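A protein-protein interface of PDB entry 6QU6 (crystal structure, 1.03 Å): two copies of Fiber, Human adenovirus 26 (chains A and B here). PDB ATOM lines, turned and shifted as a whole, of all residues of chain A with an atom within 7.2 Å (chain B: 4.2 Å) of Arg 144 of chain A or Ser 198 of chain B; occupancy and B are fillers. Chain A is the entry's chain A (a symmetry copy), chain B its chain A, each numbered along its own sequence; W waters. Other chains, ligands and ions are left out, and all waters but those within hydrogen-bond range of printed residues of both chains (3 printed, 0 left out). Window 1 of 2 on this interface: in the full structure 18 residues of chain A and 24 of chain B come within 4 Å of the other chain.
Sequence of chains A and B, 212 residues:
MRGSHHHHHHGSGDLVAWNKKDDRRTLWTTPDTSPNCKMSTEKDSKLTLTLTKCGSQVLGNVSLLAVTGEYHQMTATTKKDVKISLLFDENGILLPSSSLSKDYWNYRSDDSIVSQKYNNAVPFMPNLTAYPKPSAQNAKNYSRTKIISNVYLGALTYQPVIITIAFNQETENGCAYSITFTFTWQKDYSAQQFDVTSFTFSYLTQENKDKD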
ATOM      1  N   ASN A 127      -8.343  12.679  -4.506  1.00  0.00           N
ATOM      2  CA  ASN A 127      -7.353  11.796  -5.142  1.00  0.00           C
ATOM      3  C   ASN A 127      -5.999  12.504  -5.284  1.00  0.00           C
ATOM      4  O   ASN A 127      -5.926  13.576  -5.877  1.00  0.00           O
ATOM      5  CB  ASN A 127      -7.921  11.391  -6.501  1.00  0.00           C
ATOM      6  CG  ASN A 127      -7.105  10.319  -7.189  1.00  0.00           C
ATOM      7  OD1 ASN A 127      -6.071  10.623  -7.774  1.00  0.00           O
ATOM      8  ND2 ASN A 127      -7.572   9.080  -7.104  1.00  0.00           N
ATOM      9  N   LEU A 128      -4.927  11.864  -4.815  1.00  0.00           N
ATOM     10  CA  LEU A 128      -3.584  12.496  -4.822  1.00  0.00           C
ATOM     11  C   LEU A 128      -2.903  12.402  -6.184  1.00  0.00           C
ATOM     12  O   LEU A 128      -1.920  13.117  -6.382  1.00  0.00           O
ATOM     13  CB  LEU A 128      -2.726  11.879  -3.720  1.00  0.00           C
ATOM     14  CG  LEU A 128      -3.005  12.473  -2.335  1.00  0.00           C
ATOM     15  CD1 LEU A 128      -2.431  11.570  -1.235  1.00  0.00           C
ATOM     16  CD2 LEU A 128      -2.411  13.854  -2.208  1.00  0.00           C
ATOM     17  N   THR A 129      -3.401  11.602  -7.104  1.00  0.00           N
ATOM     18  CA  THR A 129      -2.860  11.603  -8.480  1.00  0.00           C
ATOM     19  C   THR A 129      -3.540  12.720  -9.271  1.00  0.00           C
ATOM     20  O   THR A 129      -2.864  13.497  -9.971  1.00  0.00           O
ATOM     21  CB  THR A 129      -3.012  10.242  -9.147  1.00  0.00           C
ATOM     22  OG1 THR A 129      -2.269   9.323  -8.351  1.00  0.00           O
ATOM     23  CG2 THR A 129      -2.478  10.229 -10.562  1.00  0.00           C
ATOM     24  N   ALA A 130      -4.852  12.840  -9.154  1.00  0.00           N
ATOM     25  CA  ALA A 130      -5.572  13.946  -9.814  1.00  0.00           C
ATOM     26  C   ALA A 130      -5.126  15.279  -9.228  1.00  0.00           C
ATOM     27  O   ALA A 130      -5.010  16.279  -9.966  1.00  0.00           O
ATOM     28  CB  ALA A 130      -7.051  13.776  -9.646  1.00  0.00           C
ATOM     29  N   TYR A 131      -4.978  15.299  -7.913  1.00  0.00           N
ATOM     30  CA  TYR A 131      -4.740  16.557  -7.168  1.00  0.00           C
ATOM     31  C   TYR A 131      -3.504  16.388  -6.308  1.00  0.00           C
ATOM     32  O   TYR A 131      -3.591  16.181  -5.106  1.00  0.00           O
ATOM     33  CB  TYR A 131      -5.960  16.946  -6.341  1.00  0.00           C
ATOM     34  CG  TYR A 131      -7.289  16.742  -7.019  1.00  0.00           C
ATOM     35  CD1 TYR A 131      -7.652  17.424  -8.179  1.00  0.00           C
ATOM     36  CD2 TYR A 131      -8.210  15.859  -6.490  1.00  0.00           C
ATOM     37  CE1 TYR A 131      -8.886  17.213  -8.780  1.00  0.00           C
ATOM     38  CE2 TYR A 131      -9.447  15.646  -7.069  1.00  0.00           C
ATOM     39  CZ  TYR A 131      -9.787  16.321  -8.224  1.00  0.00           C
ATOM     40  OH  TYR A 131     -11.016  16.092  -8.774  1.00  0.00           O
ATOM     41  N   PRO A 132      -2.307  16.433  -6.927  1.00  0.00           N
ATOM     42  CA  PRO A 132      -1.092  16.174  -6.177  1.00  0.00           C
ATOM     43  C   PRO A 132      -0.763  17.381  -5.303  1.00  0.00           C
ATOM     44  O   PRO A 132      -1.098  18.527  -5.611  1.00  0.00           O
ATOM     45  CB  PRO A 132      -0.021  15.971  -7.241  1.00  0.00           C
ATOM     46  CG  PRO A 132      -0.547  16.683  -8.451  1.00  0.00           C
ATOM     47  CD  PRO A 132      -2.052  16.601  -8.368  1.00  0.00           C
ATOM     48  N   ASN A 141       1.296  24.339 -10.030  1.00  0.00           N
ATOM     49  CA  ASN A 141       0.544  23.066 -10.001  1.00  0.00           C
ATOM     50  C   ASN A 141      -0.557  23.122 -11.059  1.00  0.00           C
ATOM     51  O   ASN A 141      -0.913  24.193 -11.590  1.00  0.00           O
ATOM     52  CB  ASN A 141      -0.002  22.700  -8.621  1.00  0.00           C
ATOM     53  CG  ASN A 141      -0.074  21.198  -8.412  1.00  0.00           C
ATOM     54  OD1 ASN A 141       0.164  20.413  -9.330  1.00  0.00           O
ATOM     55  ND2 ASN A 141      -0.378  20.785  -7.195  1.00  0.00           N
ATOM     56  N   TYR A 142      -1.051  21.954 -11.383  1.00  0.00           N
ATOM     57  CA  TYR A 142      -2.154  21.788 -12.335  1.00  0.00           C
ATOM     58  C   TYR A 142      -3.342  22.662 -11.912  1.00  0.00           C
ATOM     59  O   TYR A 142      -3.780  22.577 -10.752  1.00  0.00           O
ATOM     60  CB  TYR A 142      -2.503  20.297 -12.404  1.00  0.00           C
ATOM     61  CG  TYR A 142      -1.339  19.409 -12.790  1.00  0.00           C
ATOM     62  CD1 TYR A 142      -0.738  19.559 -14.028  1.00  0.00           C
ATOM     63  CD2 TYR A 142      -0.795  18.454 -11.925  1.00  0.00           C
ATOM     64  CE1 TYR A 142       0.342  18.778 -14.408  1.00  0.00           C
ATOM     65  CE2 TYR A 142       0.296  17.662 -12.288  1.00  0.00           C
ATOM     66  CZ  TYR A 142       0.859  17.837 -13.535  1.00  0.00           C
ATOM     67  OH  TYR A 142       1.911  17.066 -13.916  1.00  0.00           O
ATOM     68  N   SER A 143      -3.938  23.400 -12.840  1.00  0.00           N
ATOM     69  CA  SER A 143      -5.130  24.189 -12.508  1.00  0.00           C
ATOM     70  C   SER A 143      -6.317  23.294 -12.155  1.00  0.00           C
ATOM     71  O   SER A 143      -7.233  23.780 -11.482  1.00  0.00           O
ATOM     72  CB  SER A 143      -5.486  25.096 -13.640  1.00  0.00           C
ATOM     73  OG  SER A 143      -4.460  26.012 -13.952  1.00  0.00           O
ATOM     74  N   ARG A 144      -6.311  22.021 -12.547  1.00  0.00           N
ATOM     75  CA  ARG A 144      -7.458  21.139 -12.233  1.00  0.00           C
ATOM     76  C   ARG A 144      -7.590  20.918 -10.727  1.00  0.00           C
ATOM     77  O   ARG A 144      -8.650  20.469 -10.289  1.00  0.00           O
ATOM     78  CB  ARG A 144      -7.357  19.789 -12.940  1.00  0.00           C
ATOM     79  CG  ARG A 144      -6.211  18.918 -12.468  1.00  0.00           C
ATOM     80  CD  ARG A 144      -6.078  17.632 -13.291  1.00  0.00           C
ATOM     81  NE  ARG A 144      -5.093  16.754 -12.703  1.00  0.00           N
ATOM     82  CZ  ARG A 144      -4.523  15.683 -13.247  1.00  0.00           C
ATOM     83  NH1 ARG A 144      -4.825  15.260 -14.461  1.00  0.00           N
ATOM     84  NH2 ARG A 144      -3.617  15.024 -12.548  1.00  0.00           N
ATOM     85  N   THR A 145      -6.559  21.231  -9.942  1.00  0.00           N
ATOM     86  CA  THR A 145      -6.641  21.133  -8.473  1.00  0.00           C
ATOM     87  C   THR A 145      -7.603  22.149  -7.879  1.00  0.00           C
ATOM     88  O   THR A 145      -7.834  22.074  -6.664  1.00  0.00           O
ATOM     89  CB  THR A 145      -5.264  21.284  -7.841  1.00  0.00           C
ATOM     90  OG1 THR A 145      -4.740  22.581  -8.088  1.00  0.00           O
ATOM     91  CG2 THR A 145      -4.318  20.206  -8.298  1.00  0.00           C
ATOM     92  N   LYS A 146      -8.142  23.058  -8.679  1.00  0.00           N
ATOM     93  CA  LYS A 146      -9.072  24.075  -8.210  1.00  0.00           C
ATOM     94  C   LYS A 146     -10.355  24.042  -9.013  1.00  0.00           C
ATOM     95  O   LYS A 146     -10.388  23.673 -10.194  1.00  0.00           O
ATOM     96  CB  LYS A 146      -8.447  25.458  -8.274  1.00  0.00           C
ATOM     97  CG  LYS A 146      -7.398  25.638  -7.193  1.00  0.00           C
ATOM     98  CD  LYS A 146      -6.655  26.913  -7.285  1.00  0.00           C
ATOM     99  CE  LYS A 146      -5.724  27.143  -6.132  1.00  0.00           C
ATOM    100  NZ  LYS A 146      -4.945  28.375  -6.320  1.00  0.00           N
ATOM    101  N   ILE A 147     -11.411  24.512  -8.357  1.00  0.00           N
ATOM    102  CA  ILE A 147     -12.712  24.882  -8.938  1.00  0.00           C
ATOM    103  C   ILE A 147     -12.912  26.348  -8.624  1.00  0.00           C
ATOM    104  O   ILE A 147     -12.765  26.721  -7.460  1.00  0.00           O
ATOM    105  CB  ILE A 147     -13.861  24.048  -8.367  1.00  0.00           C
ATOM    106  CG1 ILE A 147     -13.635  22.559  -8.600  1.00  0.00           C
ATOM    107  CG2 ILE A 147     -15.196  24.509  -8.929  1.00  0.00           C
ATOM    108  CD1 ILE A 147     -14.570  21.706  -7.756  1.00  0.00           C
ATOM    109  N   ILE A 148     -13.265  27.163  -9.615  1.00  0.00           N
ATOM    110  CA  ILE A 148     -13.528  28.597  -9.375  1.00  0.00           C
ATOM    111  C   ILE A 148     -14.880  28.938  -9.960  1.00  0.00           C
ATOM    112  O   ILE A 148     -15.126  28.656 -11.145  1.00  0.00           O
ATOM    113  CB  ILE A 148     -12.425  29.480  -9.975  1.00  0.00           C
ATOM    114  CG1 ILE A 148     -11.105  29.233  -9.236  1.00  0.00           C
ATOM    115  CG2 ILE A 148     -12.829  30.941  -9.918  1.00  0.00           C
ATOM    116  CD1 ILE A 148      -9.909  29.948  -9.818  1.00  0.00           C
ATOM    117  N   ILE A 165     -12.306  26.519  -4.678  1.00  0.00           N
ATOM    118  CA  ILE A 165     -12.144  25.275  -3.922  1.00  0.00           C
ATOM    119  C   ILE A 165     -10.847  24.644  -4.386  1.00  0.00           C
ATOM    120  O   ILE A 165     -10.649  24.501  -5.587  1.00  0.00           O
ATOM    121  CB  ILE A 165     -13.321  24.326  -4.105  1.00  0.00           C
ATOM    122  CG1 ILE A 165     -14.638  25.050  -3.846  1.00  0.00           C
ATOM    123  CG2 ILE A 165     -13.143  23.128  -3.198  1.00  0.00           C
ATOM    124  CD1 ILE A 165     -15.854  24.196  -3.982  1.00  0.00           C
ATOM    125  N   PHE A 167      -7.954  21.413  -3.836  1.00  0.00           N
ATOM    126  CA  PHE A 167      -7.773  20.040  -3.340  1.00  0.00           C
ATOM    127  C   PHE A 167      -6.292  19.745  -3.181  1.00  0.00           C
ATOM    128  O   PHE A 167      -5.532  19.844  -4.148  1.00  0.00           O
ATOM    129  CB  PHE A 167      -8.398  19.056  -4.323  1.00  0.00           C
ATOM    130  CG  PHE A 167      -9.866  19.318  -4.521  1.00  0.00           C
ATOM    131  CD1 PHE A 167     -10.780  19.077  -3.509  1.00  0.00           C
ATOM    132  CD2 PHE A 167     -10.341  19.821  -5.716  1.00  0.00           C
ATOM    133  CE1 PHE A 167     -12.125  19.370  -3.655  1.00  0.00           C
ATOM    134  CE2 PHE A 167     -11.691  20.109  -5.870  1.00  0.00           C
ATOM    135  CZ  PHE A 167     -12.571  19.892  -4.831  1.00  0.00           C
ATOM    136  N   SER A 202     -17.933  18.643  -7.338  1.00  0.00           N
ATOM    137  CA  SER A 202     -17.515  17.250  -7.167  1.00  0.00           C
ATOM    138  C   SER A 202     -16.011  17.177  -7.281  1.00  0.00           C
ATOM    139  O   SER A 202     -15.363  18.095  -7.808  1.00  0.00           O
ATOM    140  CB  SER A 202     -18.187  16.320  -8.141  1.00  0.00           C
ATOM    141  OG  SER A 202     -17.630  16.431  -9.437  1.00  0.00           O
ATOM    142  N   PRO B  31      -6.149  10.095 -14.019  1.00  0.00           N
ATOM    143  CA  PRO B  31      -5.536  11.399 -13.788  1.00  0.00           C
ATOM    144  C   PRO B  31      -4.026  11.352 -14.065  1.00  0.00           C
ATOM    145  O   PRO B  31      -3.320  12.250 -13.684  1.00  0.00           O
ATOM    146  CB  PRO B  31      -5.835  11.624 -12.300  1.00  0.00           C
ATOM    147  CG  PRO B  31      -6.009  10.231 -11.695  1.00  0.00           C
ATOM    148  CD  PRO B  31      -6.046   9.234 -12.837  1.00  0.00           C
ATOM    149  N   THR B  48      -8.515  15.529 -18.694  1.00  0.00           N
ATOM    150  CA  THR B  48      -8.863  14.752 -17.498  1.00  0.00           C
ATOM    151  C   THR B  48     -10.387  14.713 -17.440  1.00  0.00           C
ATOM    152  O   THR B  48     -11.011  15.765 -17.308  1.00  0.00           O
ATOM    153  CB  THR B  48      -8.253  15.334 -16.227  1.00  0.00           C
ATOM    154  OG1 THR B  48      -6.848  15.491 -16.369  1.00  0.00           O
ATOM    155  CG2 THR B  48      -8.546  14.457 -15.033  1.00  0.00           C
ATOM    156  N   VAL B  62     -14.431  17.513 -15.517  1.00  0.00           N
ATOM    157  CA  VAL B  62     -13.530  17.675 -16.665  1.00  0.00           C
ATOM    158  C   VAL B  62     -12.547  18.811 -16.438  1.00  0.00           C
ATOM    159  O   VAL B  62     -12.887  19.854 -15.864  1.00  0.00           O
ATOM    160  CB  VAL B  62     -14.337  17.886 -17.961  1.00  0.00           C
ATOM    161  CG1 VAL B  62     -15.132  19.173 -17.954  1.00  0.00           C
ATOM    162  CG2 VAL B  62     -13.472  17.766 -19.205  1.00  0.00           C
ATOM    163  N   SER B  63     -11.365  18.652 -17.025  1.00  0.00           N
ATOM    164  CA  SER B  63     -10.358  19.720 -17.143  1.00  0.00           C
ATOM    165  C   SER B  63      -9.443  19.382 -18.318  1.00  0.00           C
ATOM    166  O   SER B  63      -9.421  18.228 -18.782  1.00  0.00           O
ATOM    167  CB  SER B  63      -9.582  19.875 -15.854  1.00  0.00           C
ATOM    168  OG  SER B  63      -8.740  18.753 -15.666  1.00  0.00           O
ATOM    169  N   VAL B 196      -6.883  24.783 -17.365  1.00  0.00           N
ATOM    170  CA  VAL B 196      -8.105  25.329 -16.757  1.00  0.00           C
ATOM    171  C   VAL B 196      -8.484  24.566 -15.489  1.00  0.00           C
ATOM    172  O   VAL B 196      -8.132  23.407 -15.274  1.00  0.00           O
ATOM    173  CB  VAL B 196      -9.284  25.363 -17.745  1.00  0.00           C
ATOM    174  CG1 VAL B 196      -9.041  26.391 -18.837  1.00  0.00           C
ATOM    175  CG2 VAL B 196      -9.596  23.995 -18.307  1.00  0.00           C
ATOM    176  N   THR B 197      -9.228  25.263 -14.651  1.00  0.00           N
ATOM    177  CA  THR B 197      -9.858  24.677 -13.477  1.00  0.00           C
ATOM    178  C   THR B 197     -10.823  23.574 -13.871  1.00  0.00           C
ATOM    179  O   THR B 197     -11.272  23.476 -15.016  1.00  0.00           O
ATOM    180  CB  THR B 197     -10.527  25.773 -12.650  1.00  0.00           C
ATOM    181  OG1 THR B 197     -11.441  26.511 -13.457  1.00  0.00           O
ATOM    182  CG2 THR B 197      -9.498  26.699 -12.038  1.00  0.00           C
ATOM    183  N   SER B 198     -11.153  22.731 -12.891  1.00  0.00           N
ATOM    184  CA  SER B 198     -12.082  21.617 -13.078  1.00  0.00           C
ATOM    185  C   SER B 198     -13.525  22.095 -13.099  1.00  0.00           C
ATOM    186  O   SER B 198     -13.903  23.042 -12.394  1.00  0.00           O
ATOM    187  CB  SER B 198     -11.882  20.605 -11.970  1.00  0.00           C
ATOM    188  OG  SER B 198     -10.639  19.937 -12.096  1.00  0.00           O
ATOM    189  N   PHE B 199     -14.351  21.390 -13.854  1.00  0.00           N
ATOM    190  CA  PHE B 199     -15.767  21.715 -14.000  1.00  0.00           C
ATOM    191  C   PHE B 199     -16.598  20.471 -13.766  1.00  0.00           C
ATOM    192  O   PHE B 199     -16.379  19.443 -14.393  1.00  0.00           O
ATOM    193  CB  PHE B 199     -16.041  22.287 -15.389  1.00  0.00           C
ATOM    194  CG  PHE B 199     -17.443  22.802 -15.547  1.00  0.00           C
ATOM    195  CD1 PHE B 199     -17.819  23.971 -14.926  1.00  0.00           C
ATOM    196  CD2 PHE B 199     -18.385  22.136 -16.314  1.00  0.00           C
ATOM    197  CE1 PHE B 199     -19.103  24.462 -15.044  1.00  0.00           C
ATOM    198  CE2 PHE B 199     -19.677  22.625 -16.439  1.00  0.00           C
ATOM    199  CZ  PHE B 199     -20.027  23.769 -15.779  1.00  0.00           C
HETATM  200  O   HOH W   1     -10.784  20.359  -8.895  1.00  0.00           O
HETATM  201  O   HOH W   2     -13.706  25.732 -12.260  1.00  0.00           O
HETATM  202  O   HOH W   3     -10.984  17.210 -11.272  1.00  0.00           O
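The backbone carbonyl oxygen of Ser 63 of chain B sits at hydrogen-bond distance from the backbone NH of Thr 48 of chain B, at 2.8 Å. N of Ala 130 of chain A is in hydrogen-bond range of OD1 of Asn 127 of chain A, at 2.9 Å. N of Thr 129 of chain A lies within hydrogen-bond range of OD1 of Asn 127 of chain A (2.9 Å). The backbone carbonyl oxygen (O) of Thr 129 of chain A lies within hydrogen-bond range of the guanidinium group (NH2) of Arg 144 of chain A, at 3.1 Å. The backbone carbonyl oxygen (O) of Ile 147 of chain A lies within hydrogen-bond range of the backbone NH (N) of Ile 165 of chain A (2.8 Å). NE of Arg 144 of chain A is in hydrogen-bond range of O of Ala 130 of chain A (2.8 Å).
Printed residues of chain B that touch a printed residue of chain A: Pro 31, Thr 48, Ser 63, Val 196, Thr 197 and Ser 198. Hydrophobic or aromatic side chains of chain B that line the printed part of chain A: Pro 31. Printed residues of chain A that touch a printed residue of chain B: Asn 127, Thr 129, Ala 130, Ser 143, Arg 144, Lys 146, Ile 147 and Ile 148. Hydrophobic or aromatic side chains of chain A that line the printed part of chain B: Ala 130, Ile 147 and Ile 148. Among the printed residues, 14 pairs touch across the chains. Among the printed residues, no Asp or Glu carboxylate lies within 4 Å of a Lys or Arg side-chain nitrogen of the other chain.
Among the printed residues, merely in contact across the chains: Asn 127 of chain A with Pro 31 of chain B, Thr 129 of chain A with Pro 31 of chain B, Ala 130 of chain A with Pro 31 of chain B, Ser 143 of chain A with Val 196 of chain B, Ser 143 of chain A with Thr 197 of chain B, Arg 144 of chain A with Ser 63 of chain B, Arg 144 of chain A with Val 196 of chain B, Lys 146 of chain A with Thr 197 of chain B, Ile 147 of chain A with Ser 198 of chain B and Ile 148 of chain A with Thr 197 of chain B.
Of the printed residues of chain B, Arg 144 of chain A touches Pro 31 (3.0 Å), Thr 48 (2.8 Å), Ser 63 (3.2 Å), Val 196 (3.6 Å) and Ser 198 (2.7 Å). Of the printed residues of chain A, Ser 198 of chain B touches Arg 144, Lys 146 and Ile 147. Of the printed residues of chain A, Thr 48 of chain B touches Arg 144 (2.8 Å). Printed residues of chain B within 4 Å of Thr 129 of chain A: Pro 31. Tyr 142 of chain A touches none of the printed residues of chain B.
OG of Ser 198 of chain B sits at hydrogen-bond distance from O of Arg 144 of chain A, at 2.7 Å. The backbone carbonyl oxygen (O) of Pro 31 of chain B sits at hydrogen-bond distance from the guanidinium group (NH2) of Arg 144 of chain A. The side-chain hydroxyl (OG1) of Thr 48 of chain B lies within hydrogen-bond range of the guanidinium group (NH1) of Arg 144 of chain A (2.8 Å). The backbone NH (N) of Ser 198 of chain B sits at hydrogen-bond distance from the backbone carbonyl oxygen (O) of Lys 146 of chain A (3.0 Å).
Water W1 bridges the backbone carbonyl oxygen of Arg 144 of chain A (2.6 Å) and the side-chain hydroxyl of Ser 198 of chain B (3.2 Å). Water W2 lies within hydrogen-bond range of the side-chain hydroxyl (OG1) of Thr 197 of chain B, the backbone carbonyl oxygen (O) of Ser 198 of chain B and the backbone NH (N) of Ile 148 of chain A. Water W3 bridges OH of Tyr 131 of chain A (2.7 Å) and OG of Ser 198 of chain B (2.9 Å).
No position is printed for both chains.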
